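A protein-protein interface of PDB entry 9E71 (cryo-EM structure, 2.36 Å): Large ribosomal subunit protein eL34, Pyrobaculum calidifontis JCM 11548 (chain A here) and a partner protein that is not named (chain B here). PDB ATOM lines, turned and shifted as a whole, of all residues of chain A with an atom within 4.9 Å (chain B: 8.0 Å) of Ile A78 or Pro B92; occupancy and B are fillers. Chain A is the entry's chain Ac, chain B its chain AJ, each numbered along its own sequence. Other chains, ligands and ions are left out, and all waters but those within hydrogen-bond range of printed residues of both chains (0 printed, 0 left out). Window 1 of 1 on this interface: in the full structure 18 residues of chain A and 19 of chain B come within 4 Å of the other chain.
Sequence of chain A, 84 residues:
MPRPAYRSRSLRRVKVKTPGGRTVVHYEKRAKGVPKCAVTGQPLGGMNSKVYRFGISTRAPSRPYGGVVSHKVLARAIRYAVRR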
ATOM      1  N   TYR A  65      11.155   9.697  31.018  1.00  0.00           N
ATOM      2  CA  TYR A  65      11.306   8.350  30.478  1.00  0.00           C
ATOM      3  C   TYR A  65      11.174   7.261  31.536  1.00  0.00           C
ATOM      4  O   TYR A  65      11.152   6.083  31.173  1.00  0.00           O
ATOM      5  CB  TYR A  65      12.623   8.182  29.708  1.00  0.00           C
ATOM      6  CG  TYR A  65      12.606   8.921  28.395  1.00  0.00           C
ATOM      7  CD1 TYR A  65      12.872  10.279  28.341  1.00  0.00           C
ATOM      8  CD2 TYR A  65      12.298   8.268  27.213  1.00  0.00           C
ATOM      9  CE1 TYR A  65      12.843  10.964  27.149  1.00  0.00           C
ATOM     10  CE2 TYR A  65      12.267   8.946  26.015  1.00  0.00           C
ATOM     11  CZ  TYR A  65      12.541  10.293  25.991  1.00  0.00           C
ATOM     12  OH  TYR A  65      12.516  10.976  24.801  1.00  0.00           O
ATOM     13  N   VAL A  73      21.808   6.464  31.939  1.00  0.00           N
ATOM     14  CA  VAL A  73      21.581   6.585  30.505  1.00  0.00           C
ATOM     15  C   VAL A  73      20.854   7.881  30.192  1.00  0.00           C
ATOM     16  O   VAL A  73      21.185   8.569  29.220  1.00  0.00           O
ATOM     17  CB  VAL A  73      20.806   5.363  29.981  1.00  0.00           C
ATOM     18  CG1 VAL A  73      20.402   5.579  28.539  1.00  0.00           C
ATOM     19  CG2 VAL A  73      21.639   4.101  30.129  1.00  0.00           C
ATOM     20  N   LEU A  74      19.865   8.242  31.015  1.00  0.00           N
ATOM     21  CA  LEU A  74      19.112   9.469  30.768  1.00  0.00           C
ATOM     22  C   LEU A  74      19.997  10.703  30.894  1.00  0.00           C
ATOM     23  O   LEU A  74      19.950  11.597  30.045  1.00  0.00           O
ATOM     24  CB  LEU A  74      17.930   9.566  31.725  1.00  0.00           C
ATOM     25  CG  LEU A  74      17.109  10.842  31.562  1.00  0.00           C
ATOM     26  CD1 LEU A  74      16.345  10.823  30.255  1.00  0.00           C
ATOM     27  CD2 LEU A  74      16.173  11.016  32.728  1.00  0.00           C
ATOM     28  N   ALA A  75      20.831  10.755  31.935  1.00  0.00           N
ATOM     29  CA  ALA A  75      21.700  11.906  32.141  1.00  0.00           C
ATOM     30  C   ALA A  75      22.732  12.026  31.029  1.00  0.00           C
ATOM     31  O   ALA A  75      22.981  13.125  30.516  1.00  0.00           O
ATOM     32  CB  ALA A  75      22.385  11.800  33.501  1.00  0.00           C
ATOM     33  N   ARG A  76      23.340  10.903  30.634  1.00  0.00           N
ATOM     34  CA  ARG A  76      24.346  10.951  29.579  1.00  0.00           C
ATOM     35  C   ARG A  76      23.728  11.339  28.240  1.00  0.00           C
ATOM     36  O   ARG A  76      24.309  12.129  27.483  1.00  0.00           O
ATOM     37  CB  ARG A  76      25.067   9.608  29.487  1.00  0.00           C
ATOM     38  CG  ARG A  76      25.740   9.357  28.160  1.00  0.00           C
ATOM     39  CD  ARG A  76      27.061  10.086  28.049  1.00  0.00           C
ATOM     40  NE  ARG A  76      27.751  10.177  29.329  1.00  0.00           N
ATOM     41  CZ  ARG A  76      28.677  11.082  29.613  1.00  0.00           C
ATOM     42  NH1 ARG A  76      29.046  11.994  28.731  1.00  0.00           N
ATOM     43  NH2 ARG A  76      29.242  11.075  30.817  1.00  0.00           N
ATOM     44  N   ALA A  77      22.538  10.810  27.938  1.00  0.00           N
ATOM     45  CA  ALA A  77      21.856  11.185  26.706  1.00  0.00           C
ATOM     46  C   ALA A  77      21.474  12.654  26.715  1.00  0.00           C
ATOM     47  O   ALA A  77      21.559  13.330  25.683  1.00  0.00           O
ATOM     48  CB  ALA A  77      20.619  10.313  26.505  1.00  0.00           C
ATOM     49  N   ILE A  78      21.053  13.168  27.872  1.00  0.00           N
ATOM     50  CA  ILE A  78      20.691  14.577  27.976  1.00  0.00           C
ATOM     51  C   ILE A  78      21.908  15.459  27.759  1.00  0.00           C
ATOM     52  O   ILE A  78      21.820  16.503  27.107  1.00  0.00           O
ATOM     53  CB  ILE A  78      20.024  14.860  29.331  1.00  0.00           C
ATOM     54  CG1 ILE A  78      18.593  14.331  29.337  1.00  0.00           C
ATOM     55  CG2 ILE A  78      20.046  16.342  29.626  1.00  0.00           C
ATOM     56  CD1 ILE A  78      17.924  14.428  30.680  1.00  0.00           C
ATOM     57  N   ARG A  79      23.058  15.060  28.306  1.00  0.00           N
ATOM     58  CA  ARG A  79      24.290  15.814  28.086  1.00  0.00           C
ATOM     59  C   ARG A  79      24.679  15.829  26.614  1.00  0.00           C
ATOM     60  O   ARG A  79      25.070  16.872  26.069  1.00  0.00           O
ATOM     61  CB  ARG A  79      25.419  15.223  28.925  1.00  0.00           C
ATOM     62  CG  ARG A  79      25.393  15.624  30.378  1.00  0.00           C
ATOM     63  CD  ARG A  79      26.592  15.063  31.111  1.00  0.00           C
ATOM     64  NE  ARG A  79      26.290  14.771  32.504  1.00  0.00           N
ATOM     65  CZ  ARG A  79      26.488  15.619  33.502  1.00  0.00           C
ATOM     66  NH1 ARG A  79      26.984  16.826  33.294  1.00  0.00           N
ATOM     67  NH2 ARG A  79      26.184  15.243  34.740  1.00  0.00           N
ATOM     68  N   TYR A  80      24.579  14.669  25.954  1.00  0.00           N
ATOM     69  CA  TYR A  80      24.910  14.591  24.534  1.00  0.00           C
ATOM     70  C   TYR A  80      23.975  15.463  23.705  1.00  0.00           C
ATOM     71  O   TYR A  80      24.412  16.170  22.791  1.00  0.00           O
ATOM     72  CB  TYR A  80      24.845  13.143  24.052  1.00  0.00           C
ATOM     73  CG  TYR A  80      26.072  12.322  24.351  1.00  0.00           C
ATOM     74  CD1 TYR A  80      27.229  12.912  24.833  1.00  0.00           C
ATOM     75  CD2 TYR A  80      26.073  10.952  24.148  1.00  0.00           C
ATOM     76  CE1 TYR A  80      28.353  12.157  25.105  1.00  0.00           C
ATOM     77  CE2 TYR A  80      27.187  10.192  24.416  1.00  0.00           C
ATOM     78  CZ  TYR A  80      28.323  10.796  24.894  1.00  0.00           C
ATOM     79  OH  TYR A  80      29.431  10.030  25.160  1.00  0.00           O
ATOM     80  N   ALA A  81      22.680  15.433  24.017  1.00  0.00           N
ATOM     81  CA  ALA A  81      21.730  16.246  23.269  1.00  0.00           C
ATOM     82  C   ALA A  81      21.944  17.730  23.536  1.00  0.00           C
ATOM     83  O   ALA A  81      21.758  18.562  22.639  1.00  0.00           O
ATOM     84  CB  ALA A  81      20.300  15.835  23.616  1.00  0.00           C
ATOM     85  N   VAL A  82      22.322  18.083  24.766  1.00  0.00           N
ATOM     86  CA  VAL A  82      22.556  19.483  25.110  1.00  0.00           C
ATOM     87  C   VAL A  82      23.745  20.026  24.336  1.00  0.00           C
ATOM     88  O   VAL A  82      23.709  21.147  23.816  1.00  0.00           O
ATOM     89  CB  VAL A  82      22.757  19.634  26.627  1.00  0.00           C
ATOM     90  CG1 VAL A  82      23.739  20.751  26.918  1.00  0.00           C
ATOM     91  CG2 VAL A  82      21.429  19.907  27.301  1.00  0.00           C
ATOM     92  N   VAL B  12      21.360  22.982  32.116  1.00  0.00           N
ATOM     93  CA  VAL B  12      20.257  22.049  31.936  1.00  0.00           C
ATOM     94  C   VAL B  12      20.374  20.976  33.003  1.00  0.00           C
ATOM     95  O   VAL B  12      21.418  20.321  33.119  1.00  0.00           O
ATOM     96  CB  VAL B  12      20.261  21.426  30.535  1.00  0.00           C
ATOM     97  CG1 VAL B  12      19.119  20.442  30.401  1.00  0.00           C
ATOM     98  CG2 VAL B  12      20.171  22.507  29.481  1.00  0.00           C
ATOM     99  N   LYS B  13      19.311  20.790  33.778  1.00  0.00           N
ATOM    100  CA  LYS B  13      19.314  19.746  34.791  1.00  0.00           C
ATOM    101  C   LYS B  13      19.252  18.374  34.133  1.00  0.00           C
ATOM    102  O   LYS B  13      18.473  18.151  33.202  1.00  0.00           O
ATOM    103  CB  LYS B  13      18.142  19.929  35.752  1.00  0.00           C
ATOM    104  CG  LYS B  13      18.289  19.138  37.031  1.00  0.00           C
ATOM    105  CD  LYS B  13      17.498  19.748  38.165  1.00  0.00           C
ATOM    106  CE  LYS B  13      17.664  18.932  39.434  1.00  0.00           C
ATOM    107  NZ  LYS B  13      17.509  19.759  40.654  1.00  0.00           N
ATOM    108  N   VAL B  14      20.081  17.450  34.614  1.00  0.00           N
ATOM    109  CA  VAL B  14      20.173  16.131  34.012  1.00  0.00           C
ATOM    110  C   VAL B  14      19.500  15.047  34.849  1.00  0.00           C
ATOM    111  O   VAL B  14      18.997  14.074  34.279  1.00  0.00           O
ATOM    112  CB  VAL B  14      21.640  15.759  33.725  1.00  0.00           C
ATOM    113  CG1 VAL B  14      22.255  16.751  32.760  1.00  0.00           C
ATOM    114  CG2 VAL B  14      22.429  15.689  35.010  1.00  0.00           C
ATOM    115  N   LEU B  15      19.465  15.180  36.170  1.00  0.00           N
ATOM    116  CA  LEU B  15      18.886  14.159  37.029  1.00  0.00           C
ATOM    117  C   LEU B  15      17.647  14.696  37.728  1.00  0.00           C
ATOM    118  O   LEU B  15      17.360  15.895  37.713  1.00  0.00           O
ATOM    119  CB  LEU B  15      19.895  13.666  38.070  1.00  0.00           C
ATOM    120  CG  LEU B  15      21.121  12.896  37.582  1.00  0.00           C
ATOM    121  CD1 LEU B  15      21.731  12.127  38.729  1.00  0.00           C
ATOM    122  CD2 LEU B  15      20.766  11.963  36.446  1.00  0.00           C
ATOM    123  N   GLY B  16      16.913  13.786  38.350  1.00  0.00           N
ATOM    124  CA  GLY B  16      15.738  14.156  39.097  1.00  0.00           C
ATOM    125  C   GLY B  16      14.521  14.368  38.220  1.00  0.00           C
ATOM    126  O   GLY B  16      14.515  14.108  37.017  1.00  0.00           O
ATOM    127  N   GLU B  18      13.092  17.199  37.362  1.00  0.00           N
ATOM    128  CA  GLU B  18      13.221  18.324  36.449  1.00  0.00           C
ATOM    129  C   GLU B  18      14.307  18.123  35.404  1.00  0.00           C
ATOM    130  O   GLU B  18      14.799  19.114  34.857  1.00  0.00           O
ATOM    131  CB  GLU B  18      13.509  19.595  37.243  1.00  0.00           C
ATOM    132  CG  GLU B  18      12.885  19.591  38.616  1.00  0.00           C
ATOM    133  CD  GLU B  18      13.587  20.527  39.570  1.00  0.00           C
ATOM    134  OE1 GLU B  18      14.036  21.601  39.130  1.00  0.00           O
ATOM    135  OE2 GLU B  18      13.716  20.181  40.761  1.00  0.00           O
ATOM    136  N   ALA B  19      14.690  16.878  35.129  1.00  0.00           N
ATOM    137  CA  ALA B  19      15.769  16.601  34.193  1.00  0.00           C
ATOM    138  C   ALA B  19      15.403  17.054  32.788  1.00  0.00           C
ATOM    139  O   ALA B  19      14.245  16.975  32.371  1.00  0.00           O
ATOM    140  CB  ALA B  19      16.092  15.110  34.195  1.00  0.00           C
ATOM    141  N   GLY B  20      16.399  17.552  32.063  1.00  0.00           N
ATOM    142  CA  GLY B  20      16.193  18.064  30.729  1.00  0.00           C
ATOM    143  C   GLY B  20      15.679  19.481  30.671  1.00  0.00           C
ATOM    144  O   GLY B  20      15.540  20.026  29.570  1.00  0.00           O
ATOM    145  N   ARG B  21      15.403  20.098  31.814  1.00  0.00           N
ATOM    146  CA  ARG B  21      14.861  21.444  31.867  1.00  0.00           C
ATOM    147  C   ARG B  21      15.980  22.457  32.050  1.00  0.00           C
ATOM    148  O   ARG B  21      16.963  22.197  32.752  1.00  0.00           O
ATOM    149  CB  ARG B  21      13.853  21.569  33.007  1.00  0.00           C
ATOM    150  CG  ARG B  21      12.413  21.414  32.576  1.00  0.00           C
ATOM    151  CD  ARG B  21      11.475  21.795  33.698  1.00  0.00           C
ATOM    152  NE  ARG B  21      10.778  20.641  34.249  1.00  0.00           N
ATOM    153  CZ  ARG B  21       9.748  20.044  33.667  1.00  0.00           C
ATOM    154  NH1 ARG B  21       9.278  20.457  32.502  1.00  0.00           N
ATOM    155  NH2 ARG B  21       9.175  19.007  34.269  1.00  0.00           N
ATOM    156  N   HIS B  54      24.960  17.358  38.662  1.00  0.00           N
ATOM    157  CA  HIS B  54      23.634  17.073  38.136  1.00  0.00           C
ATOM    158  C   HIS B  54      23.146  18.135  37.160  1.00  0.00           C
ATOM    159  O   HIS B  54      21.972  18.120  36.784  1.00  0.00           O
ATOM    160  CB  HIS B  54      22.634  16.920  39.283  1.00  0.00           C
ATOM    161  CG  HIS B  54      23.003  15.857  40.270  1.00  0.00           C
ATOM    162  ND1 HIS B  54      22.526  15.847  41.562  1.00  0.00           N
ATOM    163  CD2 HIS B  54      23.800  14.770  40.157  1.00  0.00           C
ATOM    164  CE1 HIS B  54      23.014  14.801  42.202  1.00  0.00           C
ATOM    165  NE2 HIS B  54      23.792  14.132  41.372  1.00  0.00           N
ATOM    166  N   ILE B  55      24.014  19.052  36.746  1.00  0.00           N
ATOM    167  CA  ILE B  55      23.677  20.079  35.769  1.00  0.00           C
ATOM    168  C   ILE B  55      24.721  20.056  34.668  1.00  0.00           C
ATOM    169  O   ILE B  55      25.909  19.840  34.931  1.00  0.00           O
ATOM    170  CB  ILE B  55      23.609  21.483  36.399  1.00  0.00           C
ATOM    171  CG1 ILE B  55      24.886  21.766  37.188  1.00  0.00           C
ATOM    172  CG2 ILE B  55      22.372  21.621  37.271  1.00  0.00           C
ATOM    173  CD1 ILE B  55      25.079  23.213  37.520  1.00  0.00           C
ATOM    174  N   GLU B  56      24.279  20.274  33.436  1.00  0.00           N
ATOM    175  CA  GLU B  56      25.185  20.351  32.304  1.00  0.00           C
ATOM    176  C   GLU B  56      25.206  21.774  31.779  1.00  0.00           C
ATOM    177  O   GLU B  56      24.172  22.263  31.300  1.00  0.00           O
ATOM    178  CB  GLU B  56      24.761  19.380  31.206  1.00  0.00           C
ATOM    179  CG  GLU B  56      25.611  19.462  29.953  1.00  0.00           C
ATOM    180  CD  GLU B  56      26.874  18.637  30.053  1.00  0.00           C
ATOM    181  OE1 GLU B  56      27.227  18.219  31.174  1.00  0.00           O
ATOM    182  OE2 GLU B  56      27.511  18.402  29.008  1.00  0.00           O
ATOM    183  N   ARG B  89      12.721  22.118  26.053  1.00  0.00           N
ATOM    184  CA  ARG B  89      13.256  21.035  26.871  1.00  0.00           C
ATOM    185  C   ARG B  89      14.124  20.118  26.020  1.00  0.00           C
ATOM    186  O   ARG B  89      13.754  19.760  24.899  1.00  0.00           O
ATOM    187  CB  ARG B  89      12.137  20.223  27.527  1.00  0.00           C
ATOM    188  CG  ARG B  89      11.716  20.743  28.891  1.00  0.00           C
ATOM    189  CD  ARG B  89      10.690  19.841  29.568  1.00  0.00           C
ATOM    190  NE  ARG B  89      10.201  18.774  28.706  1.00  0.00           N
ATOM    191  CZ  ARG B  89       9.149  18.876  27.904  1.00  0.00           C
ATOM    192  NH1 ARG B  89       8.440  19.993  27.835  1.00  0.00           N
ATOM    193  NH2 ARG B  89       8.799  17.834  27.156  1.00  0.00           N
ATOM    194  N   VAL B  90      15.284  19.741  26.561  1.00  0.00           N
ATOM    195  CA  VAL B  90      16.257  18.965  25.802  1.00  0.00           C
ATOM    196  C   VAL B  90      15.763  17.537  25.622  1.00  0.00           C
ATOM    197  O   VAL B  90      15.291  16.895  26.570  1.00  0.00           O
ATOM    198  CB  VAL B  90      17.627  18.999  26.494  1.00  0.00           C
ATOM    199  CG1 VAL B  90      18.595  18.072  25.786  1.00  0.00           C
ATOM    200  CG2 VAL B  90      18.168  20.412  26.507  1.00  0.00           C
ATOM    201  N   LYS B  91      15.875  17.032  24.397  1.00  0.00           N
ATOM    202  CA  LYS B  91      15.385  15.706  24.042  1.00  0.00           C
ATOM    203  C   LYS B  91      16.540  14.739  23.843  1.00  0.00           C
ATOM    204  O   LYS B  91      17.301  14.887  22.874  1.00  0.00           O
ATOM    205  CB  LYS B  91      14.538  15.777  22.775  1.00  0.00           C
ATOM    206  CG  LYS B  91      13.462  16.832  22.808  1.00  0.00           C
ATOM    207  CD  LYS B  91      12.210  16.268  23.437  1.00  0.00           C
ATOM    208  CE  LYS B  91      11.842  14.933  22.810  1.00  0.00           C
ATOM    209  NZ  LYS B  91      11.838  14.994  21.323  1.00  0.00           N
ATOM    210  N   PRO B  92      16.706  13.740  24.702  1.00  0.00           N
ATOM    211  CA  PRO B  92      17.786  12.771  24.508  1.00  0.00           C
ATOM    212  C   PRO B  92      17.494  11.826  23.354  1.00  0.00           C
ATOM    213  O   PRO B  92      16.347  11.608  22.961  1.00  0.00           O
ATOM    214  CB  PRO B  92      17.829  12.018  25.838  1.00  0.00           C
ATOM    215  CG  PRO B  92      16.457  12.131  26.371  1.00  0.00           C
ATOM    216  CD  PRO B  92      15.891  13.434  25.889  1.00  0.00           C
ATOM    217  N   LYS B  93      18.565  11.261  22.811  1.00  0.00           N
ATOM    218  CA  LYS B  93      18.495  10.233  21.776  1.00  0.00           C
ATOM    219  C   LYS B  93      18.927   8.921  22.424  1.00  0.00           C
ATOM    220  O   LYS B  93      20.104   8.560  22.408  1.00  0.00           O
ATOM    221  CB  LYS B  93      19.373  10.588  20.587  1.00  0.00           C
ATOM    222  CG  LYS B  93      19.192  12.007  20.094  1.00  0.00           C
ATOM    223  CD  LYS B  93      17.967  12.122  19.210  1.00  0.00           C
ATOM    224  CE  LYS B  93      18.313  11.900  17.749  1.00  0.00           C
ATOM    225  NZ  LYS B  93      18.498  13.184  17.023  1.00  0.00           N
ATOM    226  N   LEU B  94      17.956   8.204  22.992  1.00  0.00           N
ATOM    227  CA  LEU B  94      18.268   7.017  23.779  1.00  0.00           C
ATOM    228  C   LEU B  94      18.804   5.882  22.919  1.00  0.00           C
ATOM    229  O   LEU B  94      19.569   5.045  23.412  1.00  0.00           O
ATOM    230  CB  LEU B  94      17.029   6.561  24.543  1.00  0.00           C
ATOM    231  CG  LEU B  94      16.360   7.611  25.426  1.00  0.00           C
ATOM    232  CD1 LEU B  94      15.442   6.941  26.420  1.00  0.00           C
ATOM    233  CD2 LEU B  94      17.404   8.443  26.137  1.00  0.00           C
ATOM    234  N   PHE B  95      18.422   5.830  21.644  1.00  0.00           N
ATOM    235  CA  PHE B  95      18.849   4.737  20.782  1.00  0.00           C
ATOM    236  C   PHE B  95      20.343   4.759  20.481  1.00  0.00           C
ATOM    237  O   PHE B  95      20.898   3.715  20.127  1.00  0.00           O
ATOM    238  CB  PHE B  95      18.061   4.767  19.475  1.00  0.00           C
ATOM    239  CG  PHE B  95      16.606   4.442  19.642  1.00  0.00           C
ATOM    240  CD1 PHE B  95      16.214   3.227  20.174  1.00  0.00           C
ATOM    241  CD2 PHE B  95      15.632   5.350  19.274  1.00  0.00           C
ATOM    242  CE1 PHE B  95      14.877   2.921  20.331  1.00  0.00           C
ATOM    243  CE2 PHE B  95      14.293   5.048  19.429  1.00  0.00           C
ATOM    244  CZ  PHE B  95      13.917   3.830  19.958  1.00  0.00           C
ATOM    245  N   GLU B  96      21.001   5.906  20.610  1.00  0.00           N
ATOM    246  CA  GLU B  96      22.424   6.003  20.323  1.00  0.00           C
ATOM    247  C   GLU B  96      23.286   5.405  21.426  1.00  0.00           C
ATOM    248  O   GLU B  96      24.355   4.864  21.129  1.00  0.00           O
ATOM    249  CB  GLU B  96      22.781   7.480  20.050  1.00  0.00           C
ATOM    250  CG  GLU B  96      24.252   7.877  19.750  1.00  0.00           C
ATOM    251  CD  GLU B  96      25.154   8.013  20.975  1.00  0.00           C
ATOM    252  OE1 GLU B  96      25.892   7.060  21.299  1.00  0.00           O
ATOM    253  OE2 GLU B  96      25.122   9.083  21.616  1.00  0.00           O
ATOM    254  N   ILE B  97      22.840   5.449  22.673  1.00  0.00           N
ATOM    255  CA  ILE B  97      23.665   5.093  23.819  1.00  0.00           C
ATOM    256  C   ILE B  97      23.844   3.585  23.882  1.00  0.00           C
ATOM    257  O   ILE B  97      22.879   2.823  23.740  1.00  0.00           O
ATOM    258  CB  ILE B  97      23.052   5.626  25.125  1.00  0.00           C
ATOM    259  CG1 ILE B  97      23.027   7.151  25.097  1.00  0.00           C
ATOM    260  CG2 ILE B  97      23.834   5.123  26.321  1.00  0.00           C
ATOM    261  CD1 ILE B  97      24.282   7.777  25.629  1.00  0.00           C
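NH1 of Arg A79 lies within salt-bridge range of OE1 of Glu B56, 2.5 Å away.
The backbone carbonyl oxygen (O) of Lys B13 lies within hydrogen-bond range of the backbone NH (N) of Gly B20, 2.4 Å away.
The backbone NH (N) of Val B14 is in hydrogen-bond range of the backbone carbonyl oxygen (O) of His B54 (3.0 Å).
O of Val B12 lies within hydrogen-bond range of N of Glu B56, at 2.9 Å.
O of Gly B20 lies within hydrogen-bond range of N of Val B90, at 3.0 Å.
Pro B92 touches Tyr A65.
CD1 of Leu B94 touches CD2 of Tyr A65, 3.5 Å away.
Leu B15 touches Ala A75 (CD2 to CB, 3.4 Å).
Arg A76 touches Ile B97 (CG to CD1, 3.3 Å).
Ala A77 touches Pro B92.
CD1 of Ile A78 touches O of Val B14, 3.8 Å away.
Ile A78 touches Val B90.
N of Ile A78 touches CB of Pro B92, at 3.98 Å.
Arg A79 touches Val B14 (NH2 to CG2, 3.8 Å).
Lys B91 touches Ala A81.
Printed residues of chain B within 4 Å of Ile A78: Val B14, Gly B20, Val B90 and Pro B92.
Of the printed residues of chain A, Pro B92 touches Tyr A65, Ala A77 and Ile A78.
Ala A77 touches just these residues of chain B: Pro B92 and Leu B94.
Of the printed residues of chain B, Tyr A80 touches Glu B96 and Ile B97.
Of the printed residues of chain B, Ala A81 touches Val B90 and Lys B91.
Phe B95 touches none of the printed residues of chain A.
Val A73 touches none of the printed residues of chain B.
The nearest printed residue of chain B that does not touch Ile A78 is Ala B19 (4.02 Å).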
